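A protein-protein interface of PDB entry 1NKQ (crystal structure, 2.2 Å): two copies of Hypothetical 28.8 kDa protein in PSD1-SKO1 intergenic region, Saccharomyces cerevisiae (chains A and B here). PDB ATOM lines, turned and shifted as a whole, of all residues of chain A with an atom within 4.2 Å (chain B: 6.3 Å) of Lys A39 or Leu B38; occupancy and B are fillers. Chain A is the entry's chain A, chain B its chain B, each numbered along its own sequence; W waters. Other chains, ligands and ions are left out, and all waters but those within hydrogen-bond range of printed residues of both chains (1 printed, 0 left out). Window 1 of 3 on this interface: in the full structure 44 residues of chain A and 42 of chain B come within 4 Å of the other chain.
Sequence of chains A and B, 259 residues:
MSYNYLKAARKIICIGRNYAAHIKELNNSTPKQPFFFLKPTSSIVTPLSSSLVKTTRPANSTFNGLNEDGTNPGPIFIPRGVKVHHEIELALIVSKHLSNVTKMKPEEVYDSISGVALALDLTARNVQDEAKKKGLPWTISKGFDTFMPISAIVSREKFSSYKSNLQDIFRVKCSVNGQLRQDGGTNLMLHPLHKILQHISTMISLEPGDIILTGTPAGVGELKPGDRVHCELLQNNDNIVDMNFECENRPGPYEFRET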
ATOM      1  N   ILE A  12     -10.453  10.666   1.991  1.00  0.00           N
ATOM      2  CA  ILE A  12     -11.074   9.498   1.377  1.00  0.00           C
ATOM      3  C   ILE A  12     -11.962  10.043   0.261  1.00  0.00           C
ATOM      4  O   ILE A  12     -12.884  10.803   0.528  1.00  0.00           O
ATOM      5  CB  ILE A  12     -11.988   8.747   2.372  1.00  0.00           C
ATOM      6  CG1 ILE A  12     -11.182   8.307   3.589  1.00  0.00           C
ATOM      7  CG2 ILE A  12     -12.640   7.541   1.694  1.00  0.00           C
ATOM      8  CD1 ILE A  12     -12.032   7.766   4.707  1.00  0.00           C
ATOM      9  N   LEU A  38     -16.739  12.800  -0.945  1.00  0.00           N
ATOM     10  CA  LEU A  38     -15.777  12.523   0.121  1.00  0.00           C
ATOM     11  C   LEU A  38     -16.405  11.794   1.303  1.00  0.00           C
ATOM     12  O   LEU A  38     -17.626  11.756   1.452  1.00  0.00           O
ATOM     13  CB  LEU A  38     -15.157  13.823   0.639  1.00  0.00           C
ATOM     14  CG  LEU A  38     -14.436  14.747  -0.344  1.00  0.00           C
ATOM     15  CD1 LEU A  38     -13.943  15.988   0.385  1.00  0.00           C
ATOM     16  CD2 LEU A  38     -13.275  14.002  -0.984  1.00  0.00           C
ATOM     17  N   LYS A  39     -15.551  11.210   2.134  1.00  0.00           N
ATOM     18  CA  LYS A  39     -15.968  10.525   3.344  1.00  0.00           C
ATOM     19  C   LYS A  39     -15.001  10.972   4.427  1.00  0.00           C
ATOM     20  O   LYS A  39     -13.802  11.088   4.189  1.00  0.00           O
ATOM     21  CB  LYS A  39     -15.887   9.005   3.187  1.00  0.00           C
ATOM     22  CG  LYS A  39     -17.179   8.368   2.756  1.00  0.00           C
ATOM     23  CD  LYS A  39     -17.219   6.901   3.132  1.00  0.00           C
ATOM     24  CE  LYS A  39     -18.639   6.376   3.088  1.00  0.00           C
ATOM     25  NZ  LYS A  39     -18.689   4.909   3.245  1.00  0.00           N
ATOM     26  N   PRO A  40     -15.507  11.247   5.631  1.00  0.00           N
ATOM     27  CA  PRO A  40     -14.599  11.677   6.692  1.00  0.00           C
ATOM     28  C   PRO A  40     -13.826  10.485   7.259  1.00  0.00           C
ATOM     29  O   PRO A  40     -14.373   9.389   7.394  1.00  0.00           O
ATOM     30  CB  PRO A  40     -15.544  12.286   7.711  1.00  0.00           C
ATOM     31  CG  PRO A  40     -16.748  11.391   7.599  1.00  0.00           C
ATOM     32  CD  PRO A  40     -16.904  11.219   6.099  1.00  0.00           C
ATOM     33  N   THR A  41     -12.558  10.690   7.585  1.00  0.00           N
ATOM     34  CA  THR A  41     -11.779   9.604   8.144  1.00  0.00           C
ATOM     35  C   THR A  41     -12.395   9.203   9.473  1.00  0.00           C
ATOM     36  O   THR A  41     -12.109   8.136   9.997  1.00  0.00           O
ATOM     37  CB  THR A  41     -10.317  10.012   8.363  1.00  0.00           C
ATOM     38  OG1 THR A  41     -10.270  11.276   9.030  1.00  0.00           O
ATOM     39  CG2 THR A  41      -9.591  10.111   7.035  1.00  0.00           C
ATOM     40  N   LEU A 120     -16.239  -0.972   3.061  1.00  0.00           N
ATOM     41  CA  LEU A 120     -17.681  -0.887   2.891  1.00  0.00           C
ATOM     42  C   LEU A 120     -18.051   0.584   2.841  1.00  0.00           C
ATOM     43  O   LEU A 120     -17.686   1.357   3.722  1.00  0.00           O
ATOM     44  CB  LEU A 120     -18.434  -1.537   4.059  1.00  0.00           C
ATOM     45  CG  LEU A 120     -18.654  -3.052   4.089  1.00  0.00           C
ATOM     46  CD1 LEU A 120     -19.153  -3.459   5.464  1.00  0.00           C
ATOM     47  CD2 LEU A 120     -19.649  -3.457   3.028  1.00  0.00           C
ATOM     48  N   ASP A 121     -18.760   0.972   1.790  1.00  0.00           N
ATOM     49  CA  ASP A 121     -19.220   2.343   1.653  1.00  0.00           C
ATOM     50  C   ASP A 121     -20.681   2.361   2.109  1.00  0.00           C
ATOM     51  O   ASP A 121     -21.598   2.216   1.296  1.00  0.00           O
ATOM     52  CB  ASP A 121     -19.105   2.788   0.200  1.00  0.00           C
ATOM     53  CG  ASP A 121     -19.685   4.167  -0.031  1.00  0.00           C
ATOM     54  OD1 ASP A 121     -19.715   4.965   0.929  1.00  0.00           O
ATOM     55  OD2 ASP A 121     -20.098   4.457  -1.172  1.00  0.00           O
ATOM     56  N   LEU A 122     -20.890   2.518   3.414  1.00  0.00           N
ATOM     57  CA  LEU A 122     -22.235   2.537   3.979  1.00  0.00           C
ATOM     58  C   LEU A 122     -22.933   3.872   3.728  1.00  0.00           C
ATOM     59  O   LEU A 122     -22.334   4.944   3.854  1.00  0.00           O
ATOM     60  CB  LEU A 122     -22.187   2.220   5.482  1.00  0.00           C
ATOM     61  CG  LEU A 122     -21.532   0.867   5.817  1.00  0.00           C
ATOM     62  CD1 LEU A 122     -21.689   0.539   7.301  1.00  0.00           C
ATOM     63  CD2 LEU A 122     -22.171  -0.224   4.965  1.00  0.00           C
ATOM     64  N   THR A 139     -22.813  14.535   2.125  1.00  0.00           N
ATOM     65  CA  THR A 139     -21.913  14.393   3.271  1.00  0.00           C
ATOM     66  C   THR A 139     -22.439  13.598   4.460  1.00  0.00           C
ATOM     67  O   THR A 139     -21.844  12.589   4.839  1.00  0.00           O
ATOM     68  CB  THR A 139     -21.412  15.768   3.771  1.00  0.00           C
ATOM     69  OG1 THR A 139     -20.476  16.303   2.826  1.00  0.00           O
ATOM     70  CG2 THR A 139     -20.717  15.630   5.114  1.00  0.00           C
ATOM     71  N   LYS A 142     -23.277   9.947   3.898  1.00  0.00           N
ATOM     72  CA  LYS A 142     -22.119   9.124   3.607  1.00  0.00           C
ATOM     73  C   LYS A 142     -21.057   9.224   4.700  1.00  0.00           C
ATOM     74  O   LYS A 142     -20.081   8.474   4.686  1.00  0.00           O
ATOM     75  CB  LYS A 142     -21.506   9.553   2.278  1.00  0.00           C
ATOM     76  CG  LYS A 142     -22.331   9.222   1.049  1.00  0.00           C
ATOM     77  CD  LYS A 142     -22.086   7.792   0.612  1.00  0.00           C
ATOM     78  CE  LYS A 142     -22.643   7.516  -0.761  1.00  0.00           C
ATOM     79  NZ  LYS A 142     -22.352   6.109  -1.187  1.00  0.00           N
ATOM     80  N   PHE A 147     -19.322   4.607   9.160  1.00  0.00           N
ATOM     81  CA  PHE A 147     -19.830   4.389   7.814  1.00  0.00           C
ATOM     82  C   PHE A 147     -18.793   4.006   6.762  1.00  0.00           C
ATOM     83  O   PHE A 147     -19.075   4.001   5.564  1.00  0.00           O
ATOM     84  CB  PHE A 147     -20.693   5.572   7.363  1.00  0.00           C
ATOM     85  CG  PHE A 147     -22.152   5.419   7.732  1.00  0.00           C
ATOM     86  CD1 PHE A 147     -22.530   4.602   8.797  1.00  0.00           C
ATOM     87  CD2 PHE A 147     -23.145   6.074   7.017  1.00  0.00           C
ATOM     88  CE1 PHE A 147     -23.866   4.437   9.139  1.00  0.00           C
ATOM     89  CE2 PHE A 147     -24.492   5.916   7.357  1.00  0.00           C
ATOM     90  CZ  PHE A 147     -24.848   5.095   8.418  1.00  0.00           C
ATOM     91  N   MET A 148     -17.581   3.708   7.220  1.00  0.00           N
ATOM     92  CA  MET A 148     -16.564   3.177   6.327  1.00  0.00           C
ATOM     93  C   MET A 148     -15.815   2.017   6.979  1.00  0.00           C
ATOM     94  O   MET A 148     -14.659   2.156   7.401  1.00  0.00           O
ATOM     95  CB  MET A 148     -15.534   4.188   5.832  1.00  0.00           C
ATOM     96  CG  MET A 148     -14.682   3.450   4.794  1.00  0.00           C
ATOM     97  SD  MET A 148     -13.341   4.298   3.700  1.00  0.00           S
ATOM     98  CE  MET A 148     -11.997   4.525   5.065  1.00  0.00           C
ATOM     99  N   LYS B  11      -9.978  16.800   9.238  1.00  0.00           N
ATOM    100  CA  LYS B  11     -11.253  16.995   8.574  1.00  0.00           C
ATOM    101  C   LYS B  11     -11.687  18.462   8.516  1.00  0.00           C
ATOM    102  O   LYS B  11     -11.271  19.279   9.337  1.00  0.00           O
ATOM    103  CB  LYS B  11     -12.291  16.163   9.327  1.00  0.00           C
ATOM    104  CG  LYS B  11     -13.722  16.360   8.934  1.00  0.00           C
ATOM    105  CD  LYS B  11     -14.612  15.387   9.696  1.00  0.00           C
ATOM    106  CE  LYS B  11     -14.584  15.667  11.179  1.00  0.00           C
ATOM    107  NZ  LYS B  11     -14.913  14.453  11.961  1.00  0.00           N
ATOM    108  N   ILE B  12     -12.510  18.786   7.524  1.00  0.00           N
ATOM    109  CA  ILE B  12     -13.058  20.127   7.364  1.00  0.00           C
ATOM    110  C   ILE B  12     -14.541  19.953   7.075  1.00  0.00           C
ATOM    111  O   ILE B  12     -14.920  19.459   6.014  1.00  0.00           O
ATOM    112  CB  ILE B  12     -12.428  20.896   6.180  1.00  0.00           C
ATOM    113  CG1 ILE B  12     -10.960  21.198   6.468  1.00  0.00           C
ATOM    114  CG2 ILE B  12     -13.185  22.205   5.956  1.00  0.00           C
ATOM    115  CD1 ILE B  12     -10.219  21.749   5.307  1.00  0.00           C
ATOM    116  N   ILE B  13     -15.382  20.338   8.021  1.00  0.00           N
ATOM    117  CA  ILE B  13     -16.809  20.218   7.822  1.00  0.00           C
ATOM    118  C   ILE B  13     -17.389  21.633   7.830  1.00  0.00           C
ATOM    119  O   ILE B  13     -16.977  22.482   8.624  1.00  0.00           O
ATOM    120  CB  ILE B  13     -17.444  19.315   8.904  1.00  0.00           C
ATOM    121  CG1 ILE B  13     -18.913  19.058   8.568  1.00  0.00           C
ATOM    122  CG2 ILE B  13     -17.282  19.939  10.273  1.00  0.00           C
ATOM    123  CD1 ILE B  13     -19.416  17.689   9.020  1.00  0.00           C
ATOM    124  N   CYS B  14     -18.331  21.885   6.929  1.00  0.00           N
ATOM    125  CA  CYS B  14     -18.921  23.209   6.787  1.00  0.00           C
ATOM    126  C   CYS B  14     -20.433  23.224   6.887  1.00  0.00           C
ATOM    127  O   CYS B  14     -21.094  22.224   6.604  1.00  0.00           O
ATOM    128  CB  CYS B  14     -18.520  23.798   5.435  1.00  0.00           C
ATOM    129  SG  CYS B  14     -16.770  23.568   5.016  1.00  0.00           S
ATOM    130  N   PHE B  36     -24.750  20.259   5.941  1.00  0.00           N
ATOM    131  CA  PHE B  36     -23.297  20.300   6.048  1.00  0.00           C
ATOM    132  C   PHE B  36     -22.612  19.571   4.906  1.00  0.00           C
ATOM    133  O   PHE B  36     -23.176  18.655   4.301  1.00  0.00           O
ATOM    134  CB  PHE B  36     -22.838  19.661   7.366  1.00  0.00           C
ATOM    135  CG  PHE B  36     -23.540  20.197   8.573  1.00  0.00           C
ATOM    136  CD1 PHE B  36     -24.833  19.790   8.874  1.00  0.00           C
ATOM    137  CD2 PHE B  36     -22.917  21.124   9.403  1.00  0.00           C
ATOM    138  CE1 PHE B  36     -25.502  20.302   9.974  1.00  0.00           C
ATOM    139  CE2 PHE B  36     -23.579  21.645  10.508  1.00  0.00           C
ATOM    140  CZ  PHE B  36     -24.869  21.233  10.796  1.00  0.00           C
ATOM    141  N   PHE B  37     -21.381  19.971   4.627  1.00  0.00           N
ATOM    142  CA  PHE B  37     -20.603  19.348   3.571  1.00  0.00           C
ATOM    143  C   PHE B  37     -19.136  19.398   3.959  1.00  0.00           C
ATOM    144  O   PHE B  37     -18.731  20.250   4.745  1.00  0.00           O
ATOM    145  CB  PHE B  37     -20.839  20.071   2.240  1.00  0.00           C
ATOM    146  CG  PHE B  37     -20.452  21.521   2.258  1.00  0.00           C
ATOM    147  CD1 PHE B  37     -19.125  21.904   2.072  1.00  0.00           C
ATOM    148  CD2 PHE B  37     -21.411  22.505   2.488  1.00  0.00           C
ATOM    149  CE1 PHE B  37     -18.759  23.247   2.115  1.00  0.00           C
ATOM    150  CE2 PHE B  37     -21.057  23.851   2.534  1.00  0.00           C
ATOM    151  CZ  PHE B  37     -19.729  24.225   2.348  1.00  0.00           C
ATOM    152  N   LEU B  38     -18.349  18.468   3.422  1.00  0.00           N
ATOM    153  CA  LEU B  38     -16.921  18.411   3.712  1.00  0.00           C
ATOM    154  C   LEU B  38     -16.114  19.142   2.648  1.00  0.00           C
ATOM    155  O   LEU B  38     -16.621  19.440   1.571  1.00  0.00           O
ATOM    156  CB  LEU B  38     -16.433  16.954   3.746  1.00  0.00           C
ATOM    157  CG  LEU B  38     -17.061  15.956   4.720  1.00  0.00           C
ATOM    158  CD1 LEU B  38     -16.537  14.543   4.436  1.00  0.00           C
ATOM    159  CD2 LEU B  38     -16.740  16.373   6.140  1.00  0.00           C
ATOM    160  N   LYS B  39     -14.853  19.425   2.977  1.00  0.00           N
ATOM    161  CA  LYS B  39     -13.890  20.044   2.069  1.00  0.00           C
ATOM    162  C   LYS B  39     -12.599  19.287   2.354  1.00  0.00           C
ATOM    163  O   LYS B  39     -12.259  19.052   3.512  1.00  0.00           O
ATOM    164  CB  LYS B  39     -13.697  21.542   2.362  1.00  0.00           C
ATOM    165  CG  LYS B  39     -14.808  22.446   1.816  1.00  0.00           C
ATOM    166  CD  LYS B  39     -14.595  23.922   2.209  1.00  0.00           C
ATOM    167  CE  LYS B  39     -13.595  24.644   1.309  1.00  0.00           C
ATOM    168  NZ  LYS B  39     -14.152  24.893  -0.056  1.00  0.00           N
ATOM    169  N   PRO B  40     -11.867  18.879   1.309  1.00  0.00           N
ATOM    170  CA  PRO B  40     -10.623  18.146   1.560  1.00  0.00           C
ATOM    171  C   PRO B  40      -9.491  19.074   1.998  1.00  0.00           C
ATOM    172  O   PRO B  40      -9.371  20.189   1.502  1.00  0.00           O
ATOM    173  CB  PRO B  40     -10.347  17.491   0.224  1.00  0.00           C
ATOM    174  CG  PRO B  40     -10.776  18.560  -0.729  1.00  0.00           C
ATOM    175  CD  PRO B  40     -12.088  19.062  -0.136  1.00  0.00           C
ATOM    176  N   THR B 139     -19.040  17.676  -3.563  1.00  0.00           N
ATOM    177  CA  THR B 139     -17.599  17.490  -3.389  1.00  0.00           C
ATOM    178  C   THR B 139     -16.670  18.227  -4.337  1.00  0.00           C
ATOM    179  O   THR B 139     -15.858  19.044  -3.898  1.00  0.00           O
ATOM    180  CB  THR B 139     -17.221  15.984  -3.411  1.00  0.00           C
ATOM    181  OG1 THR B 139     -17.613  15.376  -2.171  1.00  0.00           O
ATOM    182  CG2 THR B 139     -15.722  15.805  -3.598  1.00  0.00           C
ATOM    183  N   LYS B 142     -16.763  22.049  -4.441  1.00  0.00           N
ATOM    184  CA  LYS B 142     -16.279  22.621  -3.190  1.00  0.00           C
ATOM    185  C   LYS B 142     -14.860  22.222  -2.847  1.00  0.00           C
ATOM    186  O   LYS B 142     -14.266  22.797  -1.938  1.00  0.00           O
ATOM    187  CB  LYS B 142     -17.167  22.173  -2.026  1.00  0.00           C
ATOM    188  CG  LYS B 142     -18.533  22.800  -1.973  1.00  0.00           C
ATOM    189  CD  LYS B 142     -18.456  24.227  -1.488  1.00  0.00           C
ATOM    190  CE  LYS B 142     -19.843  24.802  -1.273  1.00  0.00           C
ATOM    191  NZ  LYS B 142     -19.761  26.173  -0.709  1.00  0.00           N
ATOM    192  N   GLY B 143     -14.315  21.240  -3.563  1.00  0.00           N
ATOM    193  CA  GLY B 143     -12.989  20.765  -3.223  1.00  0.00           C
ATOM    194  C   GLY B 143     -11.789  20.976  -4.111  1.00  0.00           C
ATOM    195  O   GLY B 143     -10.735  20.433  -3.793  1.00  0.00           O
ATOM    196  N   ILE B 204     -21.459  13.213  12.842  1.00  0.00           N
ATOM    197  CA  ILE B 204     -20.067  13.034  12.472  1.00  0.00           C
ATOM    198  C   ILE B 204     -19.228  13.570  13.618  1.00  0.00           C
ATOM    199  O   ILE B 204     -19.011  14.779  13.740  1.00  0.00           O
ATOM    200  CB  ILE B 204     -19.746  13.807  11.183  1.00  0.00           C
ATOM    201  CG1 ILE B 204     -20.653  13.301  10.049  1.00  0.00           C
ATOM    202  CG2 ILE B 204     -18.273  13.656  10.834  1.00  0.00           C
ATOM    203  CD1 ILE B 204     -20.389  13.932   8.695  1.00  0.00           C
HETATM  204  O   HOH W   1     -24.786  16.471   3.744  1.00  0.00           O
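CD of Pro B40 touches CD1 of Leu A38 (3.6 Å). C of Lys A39 touches CD1 of Leu B38, at 3.9 Å. Lys B11 touches Pro A40. Leu B38 touches Pro A40. CB of Thr A139 touches O of Phe B36, 3.4 Å away. Thr A139 touches Phe B37 (OG1 to CA, 3.1 Å). Thr A139 touches Ile B204 (CG2 to CD1, 3.98 Å).
Of the 12 printed residues of chain A, 4 touch a printed residue of chain B. Hydrophobic or aromatic side chains of chain A within 4 Å of the printed part of chain B: Leu A38 and Pro A40. Of the 13 printed residues of chain B, 7 touch a printed residue of chain A. Among the printed residues, no Asp or Glu carboxylate lies within 4 Å of a Lys or Arg side-chain nitrogen of the other chain.
NZ of Lys A39 lies within salt-bridge range of OD1 of Asp A121 (2.5 Å). The backbone carbonyl oxygen (O) of Phe B37 lies within hydrogen-bond range of the backbone NH (N) of Cys B14 (2.8 Å). The backbone carbonyl oxygen (O) of Ile A12 sits at hydrogen-bond distance from the backbone NH (N) of Lys A39 (3.1 Å). The side-chain amino group (NZ) of Lys A39 lies within hydrogen-bond range of the backbone carbonyl oxygen (O) of Phe A147, 2.5 Å away.
Of the printed residues of chain B, Lys A39 touches Leu B38 (3.9 Å). Of chain A, only Lys A39, Pro A40 and Thr A139 come within 4 Å of Leu B38. Printed residues of chain A within 4 Å of Phe B36: Thr A139. Of the printed residues of chain B, Leu A38 touches Pro B40 (3.6 Å) and Thr B139 (3.0 Å). Of the printed residues of chain A, Lys B11 touches Pro A40 (3.8 Å). Of the printed residues of chain A, Pro B40 touches Leu A38. Printed residues of chain A within 4 Å of Phe B37: Thr A139 (3.1 Å). The nearest printed residue of chain A that does not touch Pro B40 is Ile A12 (7.1 Å).
The side-chain hydroxyl of Thr A139 sits at hydrogen-bond distance from the backbone NH of Leu B38, at 3.1 Å. N of Leu A38 is in hydrogen-bond range of OG1 of Thr B139.
Water W1 bridges O of Phe B36 (2.8 Å) and N of Thr A139 (3.2 Å).
Leu A38 touches Pro B40, and with the chains exchanged Pro A40 touches Leu B38. Leu A38 touches Thr B139, and with the chains exchanged Thr A139 touches Leu B38. Lys A39 touches Leu B38, but with the chains exchanged Leu A38 does not touch Lys B39 (4.1 Å). Of the 9 pairs that touch across the chains among the printed residues, 4 have their exchanged pair printed and touching as well.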
